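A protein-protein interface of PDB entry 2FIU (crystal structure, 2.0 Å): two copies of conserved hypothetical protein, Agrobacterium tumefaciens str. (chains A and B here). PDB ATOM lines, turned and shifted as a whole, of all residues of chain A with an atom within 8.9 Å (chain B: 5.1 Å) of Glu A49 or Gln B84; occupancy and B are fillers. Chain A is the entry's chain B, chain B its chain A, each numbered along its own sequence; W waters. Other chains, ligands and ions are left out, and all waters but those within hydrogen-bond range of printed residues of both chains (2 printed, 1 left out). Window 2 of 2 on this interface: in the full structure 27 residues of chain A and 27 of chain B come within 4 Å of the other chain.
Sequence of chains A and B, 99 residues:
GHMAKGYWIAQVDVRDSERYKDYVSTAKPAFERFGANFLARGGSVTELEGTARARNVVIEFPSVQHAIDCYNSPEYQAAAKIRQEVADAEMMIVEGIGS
Of the 8 printed residues of chain A, 5 touch a printed residue of chain B. Hydrophobic or aromatic side chains of chain A that line the printed part of chain B: Leu A48 and Ala A52. Among the printed residues, 10 pairs touch across the chains.
No position is printed for both chains.
Among the printed residues, pairs that only touch across the chains: Thr A46 with Met B92, Glu A49 with Glu B90, Leu A48 with Tyr B71, Gln A11 with Met B92 and Ala A52 with Met B92.
OE2 of Glu A49 sits at hydrogen-bond distance from OH of Tyr B71. The backbone carbonyl oxygen (O) of Met B91 sits at hydrogen-bond distance from the backbone NH (N) of Leu A48 (3.0 Å). NE2 of Gln B84 lies within hydrogen-bond range of OE2 of Glu A49 (2.9 Å). The side-chain carboxylate (OE1) of Glu A49 lies within salt-bridge range of the guanidinium group (NH1) of Arg B83 (2.7 Å). The backbone NH (N) of Met B91 sits at hydrogen-bond distance from the backbone carbonyl oxygen (O) of Glu A49 (2.8 Å).
Glu A49 touches just these residues of chain B: Tyr B71 (2.6 Å), Arg B83 (2.7 Å), Gln B84 (2.9 Å), Glu B90 (3.4 Å) and Met B91 (2.8 Å). Gln B84 touches one residue of chain A. Of the printed residues of chain B, Thr A46 touches Met B92 (3.2 Å). Of the printed residues of chain A, Met B92 touches Gln A11, Thr A46 and Ala A52. The nearest residue of chain B that does not touch Glu A49 is Ala B89 (4.2 Å). The nearest residue of chain A that does not touch Gln B84 is Leu A48 (6.9 Å).
The guanidinium group (NH2) of Arg B83 lies within hydrogen-bond range of the side-chain sulfur (SD) of Met B91, at 3.2 Å. N of Ala A52 lies within hydrogen-bond range of OE2 of Glu A47 (2.8 Å).
Water W2 bridges the side-chain carboxylate (OE1) of Glu A49 (2.6 Å) and the backbone carbonyl oxygen (O) of Ala B89 (3.1 Å). Water W1 bridges the side-chain amide nitrogen of Gln A11 and the side-chain sulfur of Met B92.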
ATOM      1  N   GLN A  11      18.410  -8.264 -19.742  1.00  0.00           N
ATOM      2  CA  GLN A  11      17.588  -7.593 -20.741  1.00  0.00           C
ATOM      3  C   GLN A  11      16.629  -8.663 -21.234  1.00  0.00           C
ATOM      4  O   GLN A  11      17.093  -9.685 -21.705  1.00  0.00           O
ATOM      5  CB  GLN A  11      18.445  -7.067 -21.880  1.00  0.00           C
ATOM      6  CG  GLN A  11      19.655  -6.273 -21.409  1.00  0.00           C
ATOM      7  CD  GLN A  11      20.715  -6.086 -22.476  1.00  0.00           C
ATOM      8  OE1 GLN A  11      21.809  -6.660 -22.388  1.00  0.00           O
ATOM      9  NE2 GLN A  11      20.425  -5.256 -23.453  1.00  0.00           N
ATOM     10  N   THR A  46      14.809   4.468 -22.289  1.00  0.00           N
ATOM     11  CA  THR A  46      15.059   5.387 -23.383  1.00  0.00           C
ATOM     12  C   THR A  46      16.141   4.766 -24.263  1.00  0.00           C
ATOM     13  O   THR A  46      17.305   4.644 -23.832  1.00  0.00           O
ATOM     14  CB  THR A  46      15.542   6.744 -22.856  1.00  0.00           C
ATOM     15  OG1 THR A  46      14.578   7.247 -21.937  1.00  0.00           O
ATOM     16  CG2 THR A  46      15.750   7.761 -23.984  1.00  0.00           C
ATOM     17  N   GLU A  47      15.769   4.353 -25.474  1.00  0.00           N
ATOM     18  CA  GLU A  47      16.759   3.825 -26.421  1.00  0.00           C
ATOM     19  C   GLU A  47      17.556   4.998 -26.979  1.00  0.00           C
ATOM     20  O   GLU A  47      16.983   5.997 -27.455  1.00  0.00           O
ATOM     21  CB  GLU A  47      16.108   3.088 -27.584  1.00  0.00           C
ATOM     22  CG  GLU A  47      15.170   1.945 -27.254  1.00  0.00           C
ATOM     23  CD  GLU A  47      14.730   1.188 -28.533  1.00  0.00           C
ATOM     24  OE1 GLU A  47      14.663   1.821 -29.624  1.00  0.00           O
ATOM     25  OE2 GLU A  47      14.470  -0.034 -28.452  1.00  0.00           O
ATOM     26  N   LEU A  48      18.872   4.912 -26.908  1.00  0.00           N
ATOM     27  CA  LEU A  48      19.673   5.988 -27.429  1.00  0.00           C
ATOM     28  C   LEU A  48      20.260   5.546 -28.734  1.00  0.00           C
ATOM     29  O   LEU A  48      20.176   6.260 -29.723  1.00  0.00           O
ATOM     30  CB  LEU A  48      20.775   6.385 -26.439  1.00  0.00           C
ATOM     31  CG  LEU A  48      20.299   6.945 -25.106  1.00  0.00           C
ATOM     32  CD1 LEU A  48      21.499   7.180 -24.200  1.00  0.00           C
ATOM     33  CD2 LEU A  48      19.465   8.261 -25.319  1.00  0.00           C
ATOM     34  N   GLU A  49      20.898   4.379 -28.719  1.00  0.00           N
ATOM     35  CA  GLU A  49      21.505   3.811 -29.906  1.00  0.00           C
ATOM     36  C   GLU A  49      21.225   2.332 -29.851  1.00  0.00           C
ATOM     37  O   GLU A  49      21.514   1.658 -28.836  1.00  0.00           O
ATOM     38  CB  GLU A  49      23.015   4.089 -29.957  1.00  0.00           C
ATOM     39  CG  GLU A  49      23.347   5.582 -30.066  1.00  0.00           C
ATOM     40  CD  GLU A  49      24.837   5.862 -30.098  1.00  0.00           C
ATOM     41  OE1 GLU A  49      25.617   4.921 -30.393  1.00  0.00           O
ATOM     42  OE2 GLU A  49      25.220   7.027 -29.819  1.00  0.00           O
ATOM     43  N   GLY A  50      20.627   1.832 -30.923  1.00  0.00           N
ATOM     44  CA  GLY A  50      20.276   0.415 -30.991  1.00  0.00           C
ATOM     45  C   GLY A  50      18.895   0.158 -30.425  1.00  0.00           C
ATOM     46  O   GLY A  50      18.275   1.032 -29.824  1.00  0.00           O
ATOM     47  N   THR A  51      18.413  -1.054 -30.622  1.00  0.00           N
ATOM     48  CA  THR A  51      17.114  -1.463 -30.106  1.00  0.00           C
ATOM     49  C   THR A  51      17.326  -2.183 -28.767  1.00  0.00           C
ATOM     50  O   THR A  51      18.220  -3.006 -28.631  1.00  0.00           O
ATOM     51  CB  THR A  51      16.363  -2.359 -31.130  1.00  0.00           C
ATOM     52  OG1 THR A  51      15.985  -1.556 -32.261  1.00  0.00           O
ATOM     53  CG2 THR A  51      15.099  -2.976 -30.509  1.00  0.00           C
ATOM     54  N   ALA A  52      16.525  -1.801 -27.780  1.00  0.00           N
ATOM     55  CA  ALA A  52      16.556  -2.376 -26.433  1.00  0.00           C
ATOM     56  C   ALA A  52      15.465  -3.438 -26.297  1.00  0.00           C
ATOM     57  O   ALA A  52      14.413  -3.329 -26.927  1.00  0.00           O
ATOM     58  CB  ALA A  52      16.304  -1.265 -25.424  1.00  0.00           C
ATOM     59  N   ARG B  15      36.681  -1.550 -31.955  1.00  0.00           N
ATOM     60  CA  ARG B  15      37.645  -1.888 -33.017  1.00  0.00           C
ATOM     61  C   ARG B  15      38.991  -1.163 -32.879  1.00  0.00           C
ATOM     62  O   ARG B  15      40.037  -1.776 -33.067  1.00  0.00           O
ATOM     63  CB  ARG B  15      37.060  -1.621 -34.396  1.00  0.00           C
ATOM     64  CG  ARG B  15      35.902  -2.516 -34.738  1.00  0.00           C
ATOM     65  CD  ARG B  15      35.460  -2.353 -36.187  1.00  0.00           C
ATOM     66  NE  ARG B  15      35.030  -0.995 -36.514  1.00  0.00           N
ATOM     67  CZ  ARG B  15      33.830  -0.496 -36.232  1.00  0.00           C
ATOM     68  NH1 ARG B  15      32.932  -1.235 -35.593  1.00  0.00           N
ATOM     69  NH2 ARG B  15      33.532   0.752 -36.585  1.00  0.00           N
ATOM     70  N   TYR B  71      23.421  12.951 -23.028  1.00  0.00           N
ATOM     71  CA  TYR B  71      23.509  12.326 -24.361  1.00  0.00           C
ATOM     72  C   TYR B  71      23.296  13.358 -25.487  1.00  0.00           C
ATOM     73  O   TYR B  71      24.025  13.344 -26.493  1.00  0.00           O
ATOM     74  CB  TYR B  71      22.538  11.132 -24.513  1.00  0.00           C
ATOM     75  CG  TYR B  71      22.680  10.438 -25.839  1.00  0.00           C
ATOM     76  CD1 TYR B  71      23.687   9.491 -26.046  1.00  0.00           C
ATOM     77  CD2 TYR B  71      21.863  10.770 -26.918  1.00  0.00           C
ATOM     78  CE1 TYR B  71      23.856   8.882 -27.280  1.00  0.00           C
ATOM     79  CE2 TYR B  71      22.021  10.143 -28.168  1.00  0.00           C
ATOM     80  CZ  TYR B  71      23.016   9.212 -28.341  1.00  0.00           C
ATOM     81  OH  TYR B  71      23.198   8.599 -29.582  1.00  0.00           O
ATOM     82  N   ALA B  80      30.740  11.309 -29.353  1.00  0.00           N
ATOM     83  CA  ALA B  80      30.019  10.123 -29.824  1.00  0.00           C
ATOM     84  C   ALA B  80      30.330   9.779 -31.269  1.00  0.00           C
ATOM     85  O   ALA B  80      30.313   8.601 -31.644  1.00  0.00           O
ATOM     86  CB  ALA B  80      28.531  10.313 -29.682  1.00  0.00           C
ATOM     87  N   LYS B  81      30.575  10.807 -32.083  1.00  0.00           N
ATOM     88  CA  LYS B  81      30.924  10.602 -33.494  1.00  0.00           C
ATOM     89  C   LYS B  81      32.232   9.833 -33.624  1.00  0.00           C
ATOM     90  O   LYS B  81      32.366   9.022 -34.531  1.00  0.00           O
ATOM     91  CB  LYS B  81      30.983  11.929 -34.272  1.00  0.00           C
ATOM     92  CG  LYS B  81      29.602  12.579 -34.560  1.00  0.00           C
ATOM     93  CD  LYS B  81      28.534  11.527 -34.953  1.00  0.00           C
ATOM     94  CE  LYS B  81      27.088  11.970 -34.628  1.00  0.00           C
ATOM     95  NZ  LYS B  81      26.867  12.293 -33.154  1.00  0.00           N
ATOM     96  N   ILE B  82      33.183  10.071 -32.717  1.00  0.00           N
ATOM     97  CA  ILE B  82      34.417   9.275 -32.691  1.00  0.00           C
ATOM     98  C   ILE B  82      34.056   7.828 -32.413  1.00  0.00           C
ATOM     99  O   ILE B  82      34.463   6.927 -33.147  1.00  0.00           O
ATOM    100  CB  ILE B  82      35.444   9.744 -31.625  1.00  0.00           C
ATOM    101  CG1 ILE B  82      35.856  11.202 -31.840  1.00  0.00           C
ATOM    102  CG2 ILE B  82      36.693   8.804 -31.606  1.00  0.00           C
ATOM    103  CD1 ILE B  82      36.778  11.756 -30.723  1.00  0.00           C
ATOM    104  N   ARG B  83      33.258   7.615 -31.370  1.00  0.00           N
ATOM    105  CA  ARG B  83      32.893   6.274 -30.957  1.00  0.00           C
ATOM    106  C   ARG B  83      32.156   5.535 -32.058  1.00  0.00           C
ATOM    107  O   ARG B  83      32.453   4.369 -32.323  1.00  0.00           O
ATOM    108  CB  ARG B  83      32.061   6.283 -29.673  1.00  0.00           C
ATOM    109  CG  ARG B  83      31.366   4.968 -29.426  1.00  0.00           C
ATOM    110  CD  ARG B  83      30.638   4.900 -28.088  1.00  0.00           C
ATOM    111  NE  ARG B  83      29.623   5.936 -27.882  1.00  0.00           N
ATOM    112  CZ  ARG B  83      28.501   6.088 -28.592  1.00  0.00           C
ATOM    113  NH1 ARG B  83      28.218   5.277 -29.611  1.00  0.00           N
ATOM    114  NH2 ARG B  83      27.646   7.064 -28.271  1.00  0.00           N
ATOM    115  N   GLN B  84      31.205   6.213 -32.701  1.00  0.00           N
ATOM    116  CA  GLN B  84      30.386   5.579 -33.736  1.00  0.00           C
ATOM    117  C   GLN B  84      31.239   5.145 -34.936  1.00  0.00           C
ATOM    118  O   GLN B  84      30.873   4.218 -35.658  1.00  0.00           O
ATOM    119  CB  GLN B  84      29.221   6.484 -34.158  1.00  0.00           C
ATOM    120  CG  GLN B  84      28.128   6.612 -33.089  1.00  0.00           C
ATOM    121  CD  GLN B  84      27.235   7.835 -33.273  1.00  0.00           C
ATOM    122  OE1 GLN B  84      27.377   8.600 -34.239  1.00  0.00           O
ATOM    123  NE2 GLN B  84      26.312   8.031 -32.342  1.00  0.00           N
ATOM    124  N   GLU B  85      32.382   5.800 -35.123  1.00  0.00           N
ATOM    125  CA  GLU B  85      33.355   5.394 -36.163  1.00  0.00           C
ATOM    126  C   GLU B  85      34.128   4.143 -35.791  1.00  0.00           C
ATOM    127  O   GLU B  85      34.431   3.336 -36.668  1.00  0.00           O
ATOM    128  CB  GLU B  85      34.370   6.498 -36.447  1.00  0.00           C
ATOM    129  CG  GLU B  85      34.072   7.356 -37.653  1.00  0.00           C
ATOM    130  CD  GLU B  85      35.270   8.195 -38.076  1.00  0.00           C
ATOM    131  OE1 GLU B  85      36.352   7.625 -38.389  1.00  0.00           O
ATOM    132  OE2 GLU B  85      35.132   9.438 -38.090  1.00  0.00           O
ATOM    133  N   VAL B  86      34.462   3.981 -34.506  1.00  0.00           N
ATOM    134  CA  VAL B  86      35.452   2.977 -34.099  1.00  0.00           C
ATOM    135  C   VAL B  86      34.899   1.830 -33.246  1.00  0.00           C
ATOM    136  O   VAL B  86      35.670   0.959 -32.787  1.00  0.00           O
ATOM    137  CB  VAL B  86      36.704   3.618 -33.407  1.00  0.00           C
ATOM    138  CG1 VAL B  86      37.432   4.581 -34.363  1.00  0.00           C
ATOM    139  CG2 VAL B  86      36.336   4.304 -32.072  1.00  0.00           C
ATOM    140  N   ALA B  87      33.587   1.839 -33.006  1.00  0.00           N
ATOM    141  CA  ALA B  87      32.959   0.799 -32.187  1.00  0.00           C
ATOM    142  C   ALA B  87      31.508   0.506 -32.550  1.00  0.00           C
ATOM    143  O   ALA B  87      30.792   1.365 -33.071  1.00  0.00           O
ATOM    144  CB  ALA B  87      33.065   1.149 -30.710  1.00  0.00           C
ATOM    145  N   ALA B  89      27.951  -0.422 -30.703  1.00  0.00           N
ATOM    146  CA  ALA B  89      27.434  -0.169 -29.356  1.00  0.00           C
ATOM    147  C   ALA B  89      25.922  -0.139 -29.331  1.00  0.00           C
ATOM    148  O   ALA B  89      25.291   0.400 -30.250  1.00  0.00           O
ATOM    149  CB  ALA B  89      27.968   1.145 -28.806  1.00  0.00           C
ATOM    150  N   GLU B  90      25.353  -0.703 -28.266  1.00  0.00           N
ATOM    151  CA  GLU B  90      23.964  -0.435 -27.905  1.00  0.00           C
ATOM    152  C   GLU B  90      24.021   0.426 -26.658  1.00  0.00           C
ATOM    153  O   GLU B  90      24.832   0.188 -25.750  1.00  0.00           O
ATOM    154  CB  GLU B  90      23.197  -1.727 -27.605  1.00  0.00           C
ATOM    155  CG  GLU B  90      22.871  -2.554 -28.837  1.00  0.00           C
ATOM    156  CD  GLU B  90      24.088  -3.314 -29.359  1.00  0.00           C
ATOM    157  OE1 GLU B  90      24.800  -3.953 -28.549  1.00  0.00           O
ATOM    158  OE2 GLU B  90      24.338  -3.261 -30.579  1.00  0.00           O
ATOM    159  N   MET B  91      23.178   1.439 -26.626  1.00  0.00           N
ATOM    160  CA  MET B  91      23.118   2.313 -25.481  1.00  0.00           C
ATOM    161  C   MET B  91      21.698   2.693 -25.176  1.00  0.00           C
ATOM    162  O   MET B  91      20.901   2.925 -26.088  1.00  0.00           O
ATOM    163  CB  MET B  91      23.925   3.563 -25.755  1.00  0.00           C
ATOM    164  CG  MET B  91      25.429   3.305 -25.728  1.00  0.00           C
ATOM    165  SD  MET B  91      26.182   4.805 -26.493  1.00  0.00           S
ATOM    166  CE  MET B  91      25.652   6.097 -25.277  1.00  0.00           C
ATOM    167  N   MET B  92      21.389   2.741 -23.886  1.00  0.00           N
ATOM    168  CA  MET B  92      20.053   3.025 -23.425  1.00  0.00           C
ATOM    169  C   MET B  92      20.102   3.643 -22.026  1.00  0.00           C
ATOM    170  O   MET B  92      21.121   3.549 -21.326  1.00  0.00           O
ATOM    171  CB  MET B  92      19.229   1.736 -23.412  1.00  0.00           C
ATOM    172  CG  MET B  92      19.698   0.746 -22.384  1.00  0.00           C
ATOM    173  SD  MET B  92      18.657  -0.870 -22.343  1.00  0.00           S
ATOM    174  CE  MET B  92      19.995  -2.073 -21.500  1.00  0.00           C
HETATM  175  O   HOH W   1      17.958  -4.062 -23.679  1.00  0.00           O
HETATM  176  O   HOH W   2      26.505   2.884 -31.657  1.00  0.00           O
